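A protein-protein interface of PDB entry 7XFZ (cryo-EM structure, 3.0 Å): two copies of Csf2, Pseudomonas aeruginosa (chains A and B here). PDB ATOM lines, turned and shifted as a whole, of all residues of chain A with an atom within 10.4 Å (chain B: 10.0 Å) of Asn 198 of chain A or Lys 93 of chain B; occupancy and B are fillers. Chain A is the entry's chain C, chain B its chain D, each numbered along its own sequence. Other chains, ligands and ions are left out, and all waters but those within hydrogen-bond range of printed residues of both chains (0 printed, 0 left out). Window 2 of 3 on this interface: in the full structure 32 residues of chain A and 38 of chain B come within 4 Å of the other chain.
O of Glu 195 of chain A lies within hydrogen-bond range of NZ of Lys 93 of chain B, at 3.1 Å. The backbone carbonyl oxygen (O) of Val 196 of chain A is in hydrogen-bond range of the backbone NH (N) of Leu 94 of chain B, 2.5 Å away. The backbone NH (N) of Asn 198 of chain A is in hydrogen-bond range of the backbone carbonyl oxygen (O) of Leu 94 of chain B (2.7 Å).
Among the printed residues, merely in contact across the chains: Ile 185 of chain A with Ile 96 of chain B (3.6 Å), Ile 185 of chain A with Tyr 99 of chain B (3.6 Å), Leu 188 of chain A with Tyr 99 of chain B (3.9 Å), Glu 195 of chain A with Val 88 of chain B (3.6 Å), Val 196 of chain A with Glu 84 of chain B (3.2 Å), Val 196 of chain A with Lys 93 of chain B (3.3 Å), Ile 197 of chain A with Leu 94 of chain B (3.2 Å), Ile 197 of chain A with Ile 96 of chain B (3.7 Å) and Asn 198 of chain A with Lys 93 of chain B (3.3 Å).
Printed residues of chain B within 4 Å of Glu 195 of chain A: Val 88 and Lys 93. Printed residues of chain B within 4 Å of Val 196 of chain A: Glu 84, Lys 93 and Leu 94. Ile 197 of chain A touches just these residues of chain B: Leu 94 and Ile 96. Of chain B, only Lys 93 (3.3 Å) and Leu 94 (2.7 Å) come within 4 Å of Asn 198 of chain A. Gly 200 of chain A touches none of the printed residues of chain B. No residue of chain A comes within 4 Å of Gly 91 of chain B. No residue of chain A comes within 4 Å of Asn 92 of chain B. Of chain A, only Glu 195 (3.1 Å), Val 196 (3.3 Å) and Asn 198 (3.3 Å) come within 4 Å of Lys 93 of chain B. Leu 94 of chain B touches just these residues of chain A: Val 196, Ile 197 and Asn 198. The nearest residue of chain A that does not touch Lys 93 of chain B is Ile 197 of chain A (4.1 Å).
Along chain B the printed residues that touch a printed residue of chain A span positions 84 to 99. Printed residues of chain A that touch a printed residue of chain B: Ile 185, Leu 188, Glu 195, Val 196, Ile 197 and Asn 198. Hydrophobic or aromatic side chains of chain A within 4 Å of the printed part of chain B: Ile 185, Leu 188, Val 196 and Ile 197. Among the printed residues, 12 pairs touch across the chains.
No position is printed for both chains.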
ATOM      1  N   ILE A 185      -4.927 -19.889  16.958  1.00  0.00           N
ATOM      2  CA  ILE A 185      -5.768 -19.913  18.152  1.00  0.00           C
ATOM      3  C   ILE A 185      -5.973 -18.503  18.686  1.00  0.00           C
ATOM      4  O   ILE A 185      -7.059 -18.155  19.168  1.00  0.00           O
ATOM      5  CB  ILE A 185      -5.159 -20.840  19.218  1.00  0.00           C
ATOM      6  CG1 ILE A 185      -4.962 -22.241  18.642  1.00  0.00           C
ATOM      7  CG2 ILE A 185      -6.042 -20.887  20.451  1.00  0.00           C
ATOM      8  CD1 ILE A 185      -6.226 -22.859  18.106  1.00  0.00           C
ATOM      9  N   LEU A 188      -8.868 -16.424  17.186  1.00  0.00           N
ATOM     10  CA  LEU A 188     -10.260 -16.665  17.542  1.00  0.00           C
ATOM     11  C   LEU A 188     -10.836 -15.455  18.265  1.00  0.00           C
ATOM     12  O   LEU A 188     -10.371 -15.081  19.344  1.00  0.00           O
ATOM     13  CB  LEU A 188     -10.374 -17.908  18.421  1.00  0.00           C
ATOM     14  CG  LEU A 188     -10.177 -19.260  17.736  1.00  0.00           C
ATOM     15  CD1 LEU A 188     -10.061 -20.361  18.772  1.00  0.00           C
ATOM     16  CD2 LEU A 188     -11.314 -19.547  16.776  1.00  0.00           C
ATOM     17  N   GLU A 192     -16.470 -15.725  18.867  1.00  0.00           N
ATOM     18  CA  GLU A 192     -16.291 -17.183  18.887  1.00  0.00           C
ATOM     19  C   GLU A 192     -17.255 -17.823  17.890  1.00  0.00           C
ATOM     20  O   GLU A 192     -17.030 -17.670  16.676  1.00  0.00           O
ATOM     21  CB  GLU A 192     -16.353 -17.682  20.342  1.00  0.00           C
ATOM     22  CG  GLU A 192     -17.666 -17.522  21.106  1.00  0.00           C
ATOM     23  CD  GLU A 192     -18.360 -18.846  21.361  1.00  0.00           C
ATOM     24  OE1 GLU A 192     -17.714 -19.901  21.185  1.00  0.00           O
ATOM     25  OE2 GLU A 192     -19.553 -18.830  21.729  1.00  0.00           O
ATOM     26  N   ASP A 193     -18.292 -18.543  18.325  1.00  0.00           N
ATOM     27  CA  ASP A 193     -19.196 -19.276  17.445  1.00  0.00           C
ATOM     28  C   ASP A 193     -18.433 -20.312  16.631  1.00  0.00           C
ATOM     29  O   ASP A 193     -18.760 -20.568  15.467  1.00  0.00           O
ATOM     30  CB  ASP A 193     -19.967 -18.322  16.527  1.00  0.00           C
ATOM     31  CG  ASP A 193     -20.954 -17.458  17.287  1.00  0.00           C
ATOM     32  OD1 ASP A 193     -20.869 -17.410  18.531  1.00  0.00           O
ATOM     33  OD2 ASP A 193     -21.813 -16.825  16.638  1.00  0.00           O
ATOM     34  N   VAL A 194     -17.412 -20.908  17.240  1.00  0.00           N
ATOM     35  CA  VAL A 194     -16.689 -22.039  16.671  1.00  0.00           C
ATOM     36  C   VAL A 194     -16.832 -23.208  17.635  1.00  0.00           C
ATOM     37  O   VAL A 194     -16.493 -23.093  18.820  1.00  0.00           O
ATOM     38  CB  VAL A 194     -15.214 -21.699  16.406  1.00  0.00           C
ATOM     39  CG1 VAL A 194     -15.093 -20.807  15.183  1.00  0.00           C
ATOM     40  CG2 VAL A 194     -14.595 -21.015  17.615  1.00  0.00           C
ATOM     41  N   GLU A 195     -17.352 -24.327  17.137  1.00  0.00           N
ATOM     42  CA  GLU A 195     -17.596 -25.503  17.959  1.00  0.00           C
ATOM     43  C   GLU A 195     -16.911 -26.748  17.417  1.00  0.00           C
ATOM     44  O   GLU A 195     -17.208 -27.855  17.874  1.00  0.00           O
ATOM     45  CB  GLU A 195     -19.100 -25.753  18.097  1.00  0.00           C
ATOM     46  CG  GLU A 195     -19.829 -25.961  16.782  1.00  0.00           C
ATOM     47  CD  GLU A 195     -20.222 -24.658  16.114  1.00  0.00           C
ATOM     48  OE1 GLU A 195     -19.883 -23.585  16.653  1.00  0.00           O
ATOM     49  OE2 GLU A 195     -20.871 -24.709  15.049  1.00  0.00           O
ATOM     50  N   VAL A 196     -16.011 -26.596  16.446  1.00  0.00           N
ATOM     51  CA  VAL A 196     -15.262 -27.745  15.947  1.00  0.00           C
ATOM     52  C   VAL A 196     -14.255 -28.213  16.987  1.00  0.00           C
ATOM     53  O   VAL A 196     -13.918 -29.401  17.056  1.00  0.00           O
ATOM     54  CB  VAL A 196     -14.584 -27.396  14.611  1.00  0.00           C
ATOM     55  CG1 VAL A 196     -14.190 -28.658  13.873  1.00  0.00           C
ATOM     56  CG2 VAL A 196     -15.518 -26.560  13.765  1.00  0.00           C
ATOM     57  N   ILE A 197     -13.752 -27.288  17.807  1.00  0.00           N
ATOM     58  CA  ILE A 197     -12.827 -27.658  18.868  1.00  0.00           C
ATOM     59  C   ILE A 197     -13.553 -28.499  19.907  1.00  0.00           C
ATOM     60  O   ILE A 197     -14.738 -28.281  20.195  1.00  0.00           O
ATOM     61  CB  ILE A 197     -12.207 -26.399  19.496  1.00  0.00           C
ATOM     62  CG1 ILE A 197     -11.745 -25.437  18.400  1.00  0.00           C
ATOM     63  CG2 ILE A 197     -11.047 -26.771  20.404  1.00  0.00           C
ATOM     64  CD1 ILE A 197     -10.691 -24.451  18.844  1.00  0.00           C
ATOM     65  N   ASN A 198     -12.843 -29.480  20.470  1.00  0.00           N
ATOM     66  CA  ASN A 198     -13.462 -30.394  21.427  1.00  0.00           C
ATOM     67  C   ASN A 198     -13.960 -29.656  22.663  1.00  0.00           C
ATOM     68  O   ASN A 198     -15.084 -29.891  23.122  1.00  0.00           O
ATOM     69  CB  ASN A 198     -12.471 -31.486  21.824  1.00  0.00           C
ATOM     70  CG  ASN A 198     -12.915 -32.864  21.386  1.00  0.00           C
ATOM     71  OD1 ASN A 198     -14.109 -33.139  21.280  1.00  0.00           O
ATOM     72  ND2 ASN A 198     -11.953 -33.741  21.128  1.00  0.00           N
ATOM     73  N   GLY A 199     -13.146 -28.764  23.212  1.00  0.00           N
ATOM     74  CA  GLY A 199     -13.510 -28.029  24.403  1.00  0.00           C
ATOM     75  C   GLY A 199     -14.287 -26.754  24.181  1.00  0.00           C
ATOM     76  O   GLY A 199     -14.645 -26.086  25.155  1.00  0.00           O
ATOM     77  N   GLY A 200     -14.572 -26.395  22.935  1.00  0.00           N
ATOM     78  CA  GLY A 200     -15.281 -25.149  22.685  1.00  0.00           C
ATOM     79  C   GLY A 200     -14.424 -23.951  23.045  1.00  0.00           C
ATOM     80  O   GLY A 200     -13.310 -23.780  22.539  1.00  0.00           O
ATOM     81  N   ALA A 201     -14.945 -23.104  23.931  1.00  0.00           N
ATOM     82  CA  ALA A 201     -14.258 -21.898  24.366  1.00  0.00           C
ATOM     83  C   ALA A 201     -13.393 -22.123  25.600  1.00  0.00           C
ATOM     84  O   ALA A 201     -12.832 -21.162  26.135  1.00  0.00           O
ATOM     85  CB  ALA A 201     -15.269 -20.783  24.636  1.00  0.00           C
ATOM     86  N   VAL A 202     -13.272 -23.365  26.061  1.00  0.00           N
ATOM     87  CA  VAL A 202     -12.460 -23.694  27.220  1.00  0.00           C
ATOM     88  C   VAL A 202     -11.069 -24.165  26.816  1.00  0.00           C
ATOM     89  O   VAL A 202     -10.087 -23.861  27.497  1.00  0.00           O
ATOM     90  CB  VAL A 202     -13.168 -24.748  28.098  1.00  0.00           C
ATOM     91  CG1 VAL A 202     -12.359 -25.030  29.353  1.00  0.00           C
ATOM     92  CG2 VAL A 202     -14.566 -24.281  28.459  1.00  0.00           C
ATOM     93  N   ALA A 203     -10.964 -24.907  25.711  1.00  0.00           N
ATOM     94  CA  ALA A 203      -9.656 -25.342  25.231  1.00  0.00           C
ATOM     95  C   ALA A 203      -8.820 -24.162  24.755  1.00  0.00           C
ATOM     96  O   ALA A 203      -7.608 -24.110  25.006  1.00  0.00           O
ATOM     97  CB  ALA A 203      -9.824 -26.366  24.111  1.00  0.00           C
ATOM     98  N   ALA A 204      -9.446 -23.209  24.061  1.00  0.00           N
ATOM     99  CA  ALA A 204      -8.720 -22.037  23.580  1.00  0.00           C
ATOM    100  C   ALA A 204      -8.164 -21.221  24.739  1.00  0.00           C
ATOM    101  O   ALA A 204      -7.024 -20.742  24.683  1.00  0.00           O
ATOM    102  CB  ALA A 204      -9.635 -21.180  22.709  1.00  0.00           C
ATOM    103  N   ILE B  83     -14.781 -27.649   4.469  1.00  0.00           N
ATOM    104  CA  ILE B  83     -14.401 -28.703   5.404  1.00  0.00           C
ATOM    105  C   ILE B  83     -15.076 -28.502   6.756  1.00  0.00           C
ATOM    106  O   ILE B  83     -15.538 -29.464   7.379  1.00  0.00           O
ATOM    107  CB  ILE B  83     -12.870 -28.768   5.543  1.00  0.00           C
ATOM    108  CG1 ILE B  83     -12.216 -28.939   4.173  1.00  0.00           C
ATOM    109  CG2 ILE B  83     -12.467 -29.903   6.463  1.00  0.00           C
ATOM    110  CD1 ILE B  83     -12.568 -30.235   3.488  1.00  0.00           C
ATOM    111  N   GLU B  84     -15.123 -27.263   7.242  1.00  0.00           N
ATOM    112  CA  GLU B  84     -15.644 -27.010   8.585  1.00  0.00           C
ATOM    113  C   GLU B  84     -17.111 -27.398   8.737  1.00  0.00           C
ATOM    114  O   GLU B  84     -17.438 -28.109   9.704  1.00  0.00           O
ATOM    115  CB  GLU B  84     -15.412 -25.540   8.950  1.00  0.00           C
ATOM    116  CG  GLU B  84     -15.598 -25.186  10.407  1.00  0.00           C
ATOM    117  CD  GLU B  84     -14.291 -24.786  11.065  1.00  0.00           C
ATOM    118  OE1 GLU B  84     -13.221 -25.129  10.521  1.00  0.00           O
ATOM    119  OE2 GLU B  84     -14.331 -24.115  12.118  1.00  0.00           O
ATOM    120  N   PRO B  85     -18.037 -26.972   7.864  1.00  0.00           N
ATOM    121  CA  PRO B  85     -19.437 -27.389   8.052  1.00  0.00           C
ATOM    122  C   PRO B  85     -19.652 -28.884   7.909  1.00  0.00           C
ATOM    123  O   PRO B  85     -20.490 -29.454   8.617  1.00  0.00           O
ATOM    124  CB  PRO B  85     -20.181 -26.599   6.965  1.00  0.00           C
ATOM    125  CG  PRO B  85     -19.281 -25.462   6.641  1.00  0.00           C
ATOM    126  CD  PRO B  85     -17.916 -26.041   6.730  1.00  0.00           C
ATOM    127  N   ALA B  86     -18.920 -29.537   7.005  1.00  0.00           N
ATOM    128  CA  ALA B  86     -19.050 -30.983   6.859  1.00  0.00           C
ATOM    129  C   ALA B  86     -18.525 -31.710   8.090  1.00  0.00           C
ATOM    130  O   ALA B  86     -19.100 -32.716   8.520  1.00  0.00           O
ATOM    131  CB  ALA B  86     -18.316 -31.453   5.604  1.00  0.00           C
ATOM    132  N   LEU B  87     -17.427 -31.219   8.664  1.00  0.00           N
ATOM    133  CA  LEU B  87     -16.866 -31.847   9.854  1.00  0.00           C
ATOM    134  C   LEU B  87     -17.767 -31.652  11.064  1.00  0.00           C
ATOM    135  O   LEU B  87     -18.061 -32.613  11.780  1.00  0.00           O
ATOM    136  CB  LEU B  87     -15.470 -31.290  10.132  1.00  0.00           C
ATOM    137  CG  LEU B  87     -14.459 -32.208  10.824  1.00  0.00           C
ATOM    138  CD1 LEU B  87     -14.697 -33.661  10.464  1.00  0.00           C
ATOM    139  CD2 LEU B  87     -13.041 -31.794  10.478  1.00  0.00           C
ATOM    140  N   VAL B  88     -18.219 -30.418  11.308  1.00  0.00           N
ATOM    141  CA  VAL B  88     -18.999 -30.141  12.512  1.00  0.00           C
ATOM    142  C   VAL B  88     -20.340 -30.863  12.459  1.00  0.00           C
ATOM    143  O   VAL B  88     -20.879 -31.283  13.491  1.00  0.00           O
ATOM    144  CB  VAL B  88     -19.171 -28.623  12.715  1.00  0.00           C
ATOM    145  CG1 VAL B  88     -20.020 -28.013  11.614  1.00  0.00           C
ATOM    146  CG2 VAL B  88     -19.779 -28.339  14.074  1.00  0.00           C
ATOM    147  N   GLU B  89     -20.898 -31.020  11.263  1.00  0.00           N
ATOM    148  CA  GLU B  89     -22.091 -31.834  11.098  1.00  0.00           C
ATOM    149  C   GLU B  89     -21.766 -33.283  11.436  1.00  0.00           C
ATOM    150  O   GLU B  89     -20.612 -33.710  11.340  1.00  0.00           O
ATOM    151  CB  GLU B  89     -22.614 -31.704   9.667  1.00  0.00           C
ATOM    152  CG  GLU B  89     -24.047 -32.150   9.453  1.00  0.00           C
ATOM    153  CD  GLU B  89     -24.158 -33.634   9.194  1.00  0.00           C
ATOM    154  OE1 GLU B  89     -23.146 -34.237   8.782  1.00  0.00           O
ATOM    155  OE2 GLU B  89     -25.254 -34.196   9.400  1.00  0.00           O
ATOM    156  N   LYS B  90     -22.783 -34.025  11.881  1.00  0.00           N
ATOM    157  CA  LYS B  90     -22.662 -35.425  12.310  1.00  0.00           C
ATOM    158  C   LYS B  90     -21.589 -35.599  13.391  1.00  0.00           C
ATOM    159  O   LYS B  90     -20.995 -36.668  13.535  1.00  0.00           O
ATOM    160  CB  LYS B  90     -22.427 -36.370  11.118  1.00  0.00           C
ATOM    161  CG  LYS B  90     -21.004 -36.496  10.573  1.00  0.00           C
ATOM    162  CD  LYS B  90     -20.998 -36.888   9.106  1.00  0.00           C
ATOM    163  CE  LYS B  90     -19.577 -37.053   8.586  1.00  0.00           C
ATOM    164  NZ  LYS B  90     -19.097 -35.845   7.861  1.00  0.00           N
ATOM    165  N   GLY B  91     -21.377 -34.559  14.189  1.00  0.00           N
ATOM    166  CA  GLY B  91     -20.427 -34.656  15.285  1.00  0.00           C
ATOM    167  C   GLY B  91     -19.025 -34.320  14.819  1.00  0.00           C
ATOM    168  O   GLY B  91     -18.783 -33.258  14.235  1.00  0.00           O
ATOM    169  N   ASN B  92     -18.081 -35.222  15.100  1.00  0.00           N
ATOM    170  CA  ASN B  92     -16.709 -35.129  14.593  1.00  0.00           C
ATOM    171  C   ASN B  92     -16.034 -33.818  15.000  1.00  0.00           C
ATOM    172  O   ASN B  92     -15.719 -32.968  14.166  1.00  0.00           O
ATOM    173  CB  ASN B  92     -16.674 -35.312  13.075  1.00  0.00           C
ATOM    174  CG  ASN B  92     -16.946 -36.739  12.657  1.00  0.00           C
ATOM    175  OD1 ASN B  92     -16.652 -37.678  13.392  1.00  0.00           O
ATOM    176  ND2 ASN B  92     -17.505 -36.910  11.466  1.00  0.00           N
ATOM    177  N   LYS B  93     -15.819 -33.656  16.301  1.00  0.00           N
ATOM    178  CA  LYS B  93     -15.059 -32.517  16.794  1.00  0.00           C
ATOM    179  C   LYS B  93     -13.567 -32.721  16.554  1.00  0.00           C
ATOM    180  O   LYS B  93     -13.078 -33.850  16.457  1.00  0.00           O
ATOM    181  CB  LYS B  93     -15.317 -32.305  18.285  1.00  0.00           C
ATOM    182  CG  LYS B  93     -16.780 -32.150  18.650  1.00  0.00           C
ATOM    183  CD  LYS B  93     -17.460 -31.103  17.790  1.00  0.00           C
ATOM    184  CE  LYS B  93     -18.741 -30.623  18.438  1.00  0.00           C
ATOM    185  NZ  LYS B  93     -18.472 -30.008  19.763  1.00  0.00           N
ATOM    186  N   LEU B  94     -12.841 -31.612  16.467  1.00  0.00           N
ATOM    187  CA  LEU B  94     -11.390 -31.620  16.333  1.00  0.00           C
ATOM    188  C   LEU B  94     -10.758 -31.218  17.657  1.00  0.00           C
ATOM    189  O   LEU B  94     -11.336 -30.428  18.408  1.00  0.00           O
ATOM    190  CB  LEU B  94     -10.929 -30.666  15.229  1.00  0.00           C
ATOM    191  CG  LEU B  94     -11.058 -31.132  13.781  1.00  0.00           C
ATOM    192  CD1 LEU B  94     -10.698 -30.000  12.836  1.00  0.00           C
ATOM    193  CD2 LEU B  94     -10.173 -32.334  13.536  1.00  0.00           C
ATOM    194  N   SER B  95      -9.581 -31.764  17.943  1.00  0.00           N
ATOM    195  CA  SER B  95      -8.830 -31.310  19.100  1.00  0.00           C
ATOM    196  C   SER B  95      -8.171 -29.965  18.794  1.00  0.00           C
ATOM    197  O   SER B  95      -8.126 -29.509  17.651  1.00  0.00           O
ATOM    198  CB  SER B  95      -7.784 -32.346  19.503  1.00  0.00           C
ATOM    199  OG  SER B  95      -6.562 -32.119  18.831  1.00  0.00           O
ATOM    200  N   ILE B  96      -7.664 -29.319  19.846  1.00  0.00           N
ATOM    201  CA  ILE B  96      -7.044 -28.009  19.676  1.00  0.00           C
ATOM    202  C   ILE B  96      -5.764 -28.122  18.851  1.00  0.00           C
ATOM    203  O   ILE B  96      -5.493 -27.288  17.976  1.00  0.00           O
ATOM    204  CB  ILE B  96      -6.806 -27.353  21.051  1.00  0.00           C
ATOM    205  CG1 ILE B  96      -6.390 -25.891  20.899  1.00  0.00           C
ATOM    206  CG2 ILE B  96      -5.804 -28.138  21.888  1.00  0.00           C
ATOM    207  CD1 ILE B  96      -7.554 -24.955  20.737  1.00  0.00           C
ATOM    208  N   GLY B  97      -4.971 -29.168  19.095  1.00  0.00           N
ATOM    209  CA  GLY B  97      -3.767 -29.370  18.309  1.00  0.00           C
ATOM    210  C   GLY B  97      -4.064 -29.654  16.851  1.00  0.00           C
ATOM    211  O   GLY B  97      -3.365 -29.166  15.962  1.00  0.00           O
ATOM    212  N   ALA B  98      -5.106 -30.446  16.583  1.00  0.00           N
ATOM    213  CA  ALA B  98      -5.503 -30.705  15.203  1.00  0.00           C
ATOM    214  C   ALA B  98      -5.992 -29.434  14.522  1.00  0.00           C
ATOM    215  O   ALA B  98      -5.728 -29.217  13.336  1.00  0.00           O
ATOM    216  CB  ALA B  98      -6.578 -31.787  15.161  1.00  0.00           C
ATOM    217  N   TYR B  99      -6.713 -28.583  15.256  1.00  0.00           N
ATOM    218  CA  TYR B  99      -7.143 -27.301  14.707  1.00  0.00           C
ATOM    219  C   TYR B  99      -5.946 -26.440  14.316  1.00  0.00           C
ATOM    220  O   TYR B  99      -5.885 -25.910  13.196  1.00  0.00           O
ATOM    221  CB  TYR B  99      -8.012 -26.579  15.736  1.00  0.00           C
ATOM    222  CG  TYR B  99      -8.779 -25.384  15.220  1.00  0.00           C
ATOM    223  CD1 TYR B  99      -9.978 -25.544  14.543  1.00  0.00           C
ATOM    224  CD2 TYR B  99      -8.311 -24.094  15.429  1.00  0.00           C
ATOM    225  CE1 TYR B  99     -10.686 -24.456  14.082  1.00  0.00           C
ATOM    226  CE2 TYR B  99      -9.011 -23.000  14.969  1.00  0.00           C
ATOM    227  CZ  TYR B  99     -10.197 -23.187  14.297  1.00  0.00           C
ATOM    228  OH  TYR B  99     -10.900 -22.097  13.836  1.00  0.00           O
ATOM    229  N   ALA B 100      -4.975 -26.308  15.223  1.00  0.00           N
ATOM    230  CA  ALA B 100      -3.788 -25.513  14.922  1.00  0.00           C
ATOM    231  C   ALA B 100      -3.007 -26.107  13.757  1.00  0.00           C
ATOM    232  O   ALA B 100      -2.495 -25.373  12.905  1.00  0.00           O
ATOM    233  CB  ALA B 100      -2.904 -25.402  16.162  1.00  0.00           C
ATOM    234  N   LEU B 333     -15.607 -37.791   4.991  1.00  0.00           N
ATOM    235  CA  LEU B 333     -14.487 -37.288   5.774  1.00  0.00           C
ATOM    236  C   LEU B 333     -14.699 -37.564   7.258  1.00  0.00           C
ATOM    237  O   LEU B 333     -15.824 -37.526   7.762  1.00  0.00           O
ATOM    238  CB  LEU B 333     -14.283 -35.789   5.532  1.00  0.00           C
ATOM    239  CG  LEU B 333     -15.457 -34.813   5.648  1.00  0.00           C
ATOM    240  CD1 LEU B 333     -15.696 -34.379   7.079  1.00  0.00           C
ATOM    241  CD2 LEU B 333     -15.193 -33.595   4.783  1.00  0.00           C
ATOM    242  N   SER B 334     -13.603 -37.851   7.958  1.00  0.00           N
ATOM    243  CA  SER B 334     -13.630 -38.144   9.383  1.00  0.00           C
ATOM    244  C   SER B 334     -12.467 -37.440  10.067  1.00  0.00           C
ATOM    245  O   SER B 334     -11.473 -37.079   9.435  1.00  0.00           O
ATOM    246  CB  SER B 334     -13.563 -39.652   9.649  1.00  0.00           C
ATOM    247  OG  SER B 334     -13.635 -39.925  11.036  1.00  0.00           O
ATOM    248  N   SER B 335     -12.603 -37.249  11.378  1.00  0.00           N
ATOM    249  CA  SER B 335     -11.594 -36.533  12.147  1.00  0.00           C
ATOM    250  C   SER B 335     -10.457 -37.425  12.628  1.00  0.00           C
ATOM    251  O   SER B 335      -9.536 -36.922  13.277  1.00  0.00           O
ATOM    252  CB  SER B 335     -12.244 -35.844  13.346  1.00  0.00           C
ATOM    253  OG  SER B 335     -12.988 -36.768  14.118  1.00  0.00           O
ATOM    254  N   LYS B 336     -10.501 -38.727  12.341  1.00  0.00           N
ATOM    255  CA  LYS B 336      -9.426 -39.619  12.763  1.00  0.00           C
ATOM    256  C   LYS B 336      -8.114 -39.281  12.061  1.00  0.00           C
ATOM    257  O   LYS B 336      -7.042 -39.294  12.682  1.00  0.00           O
ATOM    258  CB  LYS B 336      -9.827 -41.069  12.499  1.00  0.00           C
ATOM    259  CG  LYS B 336      -8.696 -42.069  12.634  1.00  0.00           C
ATOM    260  CD  LYS B 336      -9.041 -43.376  11.941  1.00  0.00           C
ATOM    261  CE  LYS B 336      -8.786 -43.291  10.444  1.00  0.00           C
ATOM    262  NZ  LYS B 336      -7.332 -43.302  10.121  1.00  0.00           N
ATOM    263  N   GLU B 337      -8.182 -38.977  10.762  1.00  0.00           N
ATOM    264  CA  GLU B 337      -6.975 -38.655  10.007  1.00  0.00           C
ATOM    265  C   GLU B 337      -6.312 -37.391  10.533  1.00  0.00           C
ATOM    266  O   GLU B 337      -5.081 -37.307  10.590  1.00  0.00           O
ATOM    267  CB  GLU B 337      -7.307 -38.504   8.524  1.00  0.00           C
ATOM    268  CG  GLU B 337      -6.966 -39.718   7.684  1.00  0.00           C
ATOM    269  CD  GLU B 337      -8.118 -40.693   7.580  1.00  0.00           C
ATOM    270  OE1 GLU B 337      -7.873 -41.868   7.236  1.00  0.00           O
ATOM    271  OE2 GLU B 337      -9.268 -40.286   7.845  1.00  0.00           O
ATOM    272  N   PHE B 338      -7.110 -36.390  10.909  1.00  0.00           N
ATOM    273  CA  PHE B 338      -6.544 -35.162  11.457  1.00  0.00           C
ATOM    274  C   PHE B 338      -5.797 -35.429  12.756  1.00  0.00           C
ATOM    275  O   PHE B 338      -4.702 -34.898  12.971  1.00  0.00           O
ATOM    276  CB  PHE B 338      -7.645 -34.128  11.680  1.00  0.00           C
ATOM    277  CG  PHE B 338      -8.303 -33.660  10.417  1.00  0.00           C
ATOM    278  CD1 PHE B 338      -9.407 -34.319   9.912  1.00  0.00           C
ATOM    279  CD2 PHE B 338      -7.819 -32.558   9.738  1.00  0.00           C
ATOM    280  CE1 PHE B 338     -10.014 -33.888   8.753  1.00  0.00           C
ATOM    281  CE2 PHE B 338      -8.423 -32.124   8.580  1.00  0.00           C
ATOM    282  CZ  PHE B 338      -9.522 -32.790   8.087  1.00  0.00           C
ATOM    283  N   GLU B 339      -6.376 -36.249  13.636  1.00  0.00           N
ATOM    284  CA  GLU B 339      -5.701 -36.583  14.886  1.00  0.00           C
ATOM    285  C   GLU B 339      -4.417 -37.359  14.630  1.00  0.00           C
ATOM    286  O   GLU B 339      -3.398 -37.122  15.288  1.00  0.00           O
ATOM    287  CB  GLU B 339      -6.633 -37.382  15.794  1.00  0.00           C
ATOM    288  CG  GLU B 339      -7.994 -36.748  16.016  1.00  0.00           C
ATOM    289  CD  GLU B 339      -7.926 -35.475  16.831  1.00  0.00           C
ATOM    290  OE1 GLU B 339      -8.890 -34.684  16.776  1.00  0.00           O
ATOM    291  OE2 GLU B 339      -6.916 -35.268  17.535  1.00  0.00           O
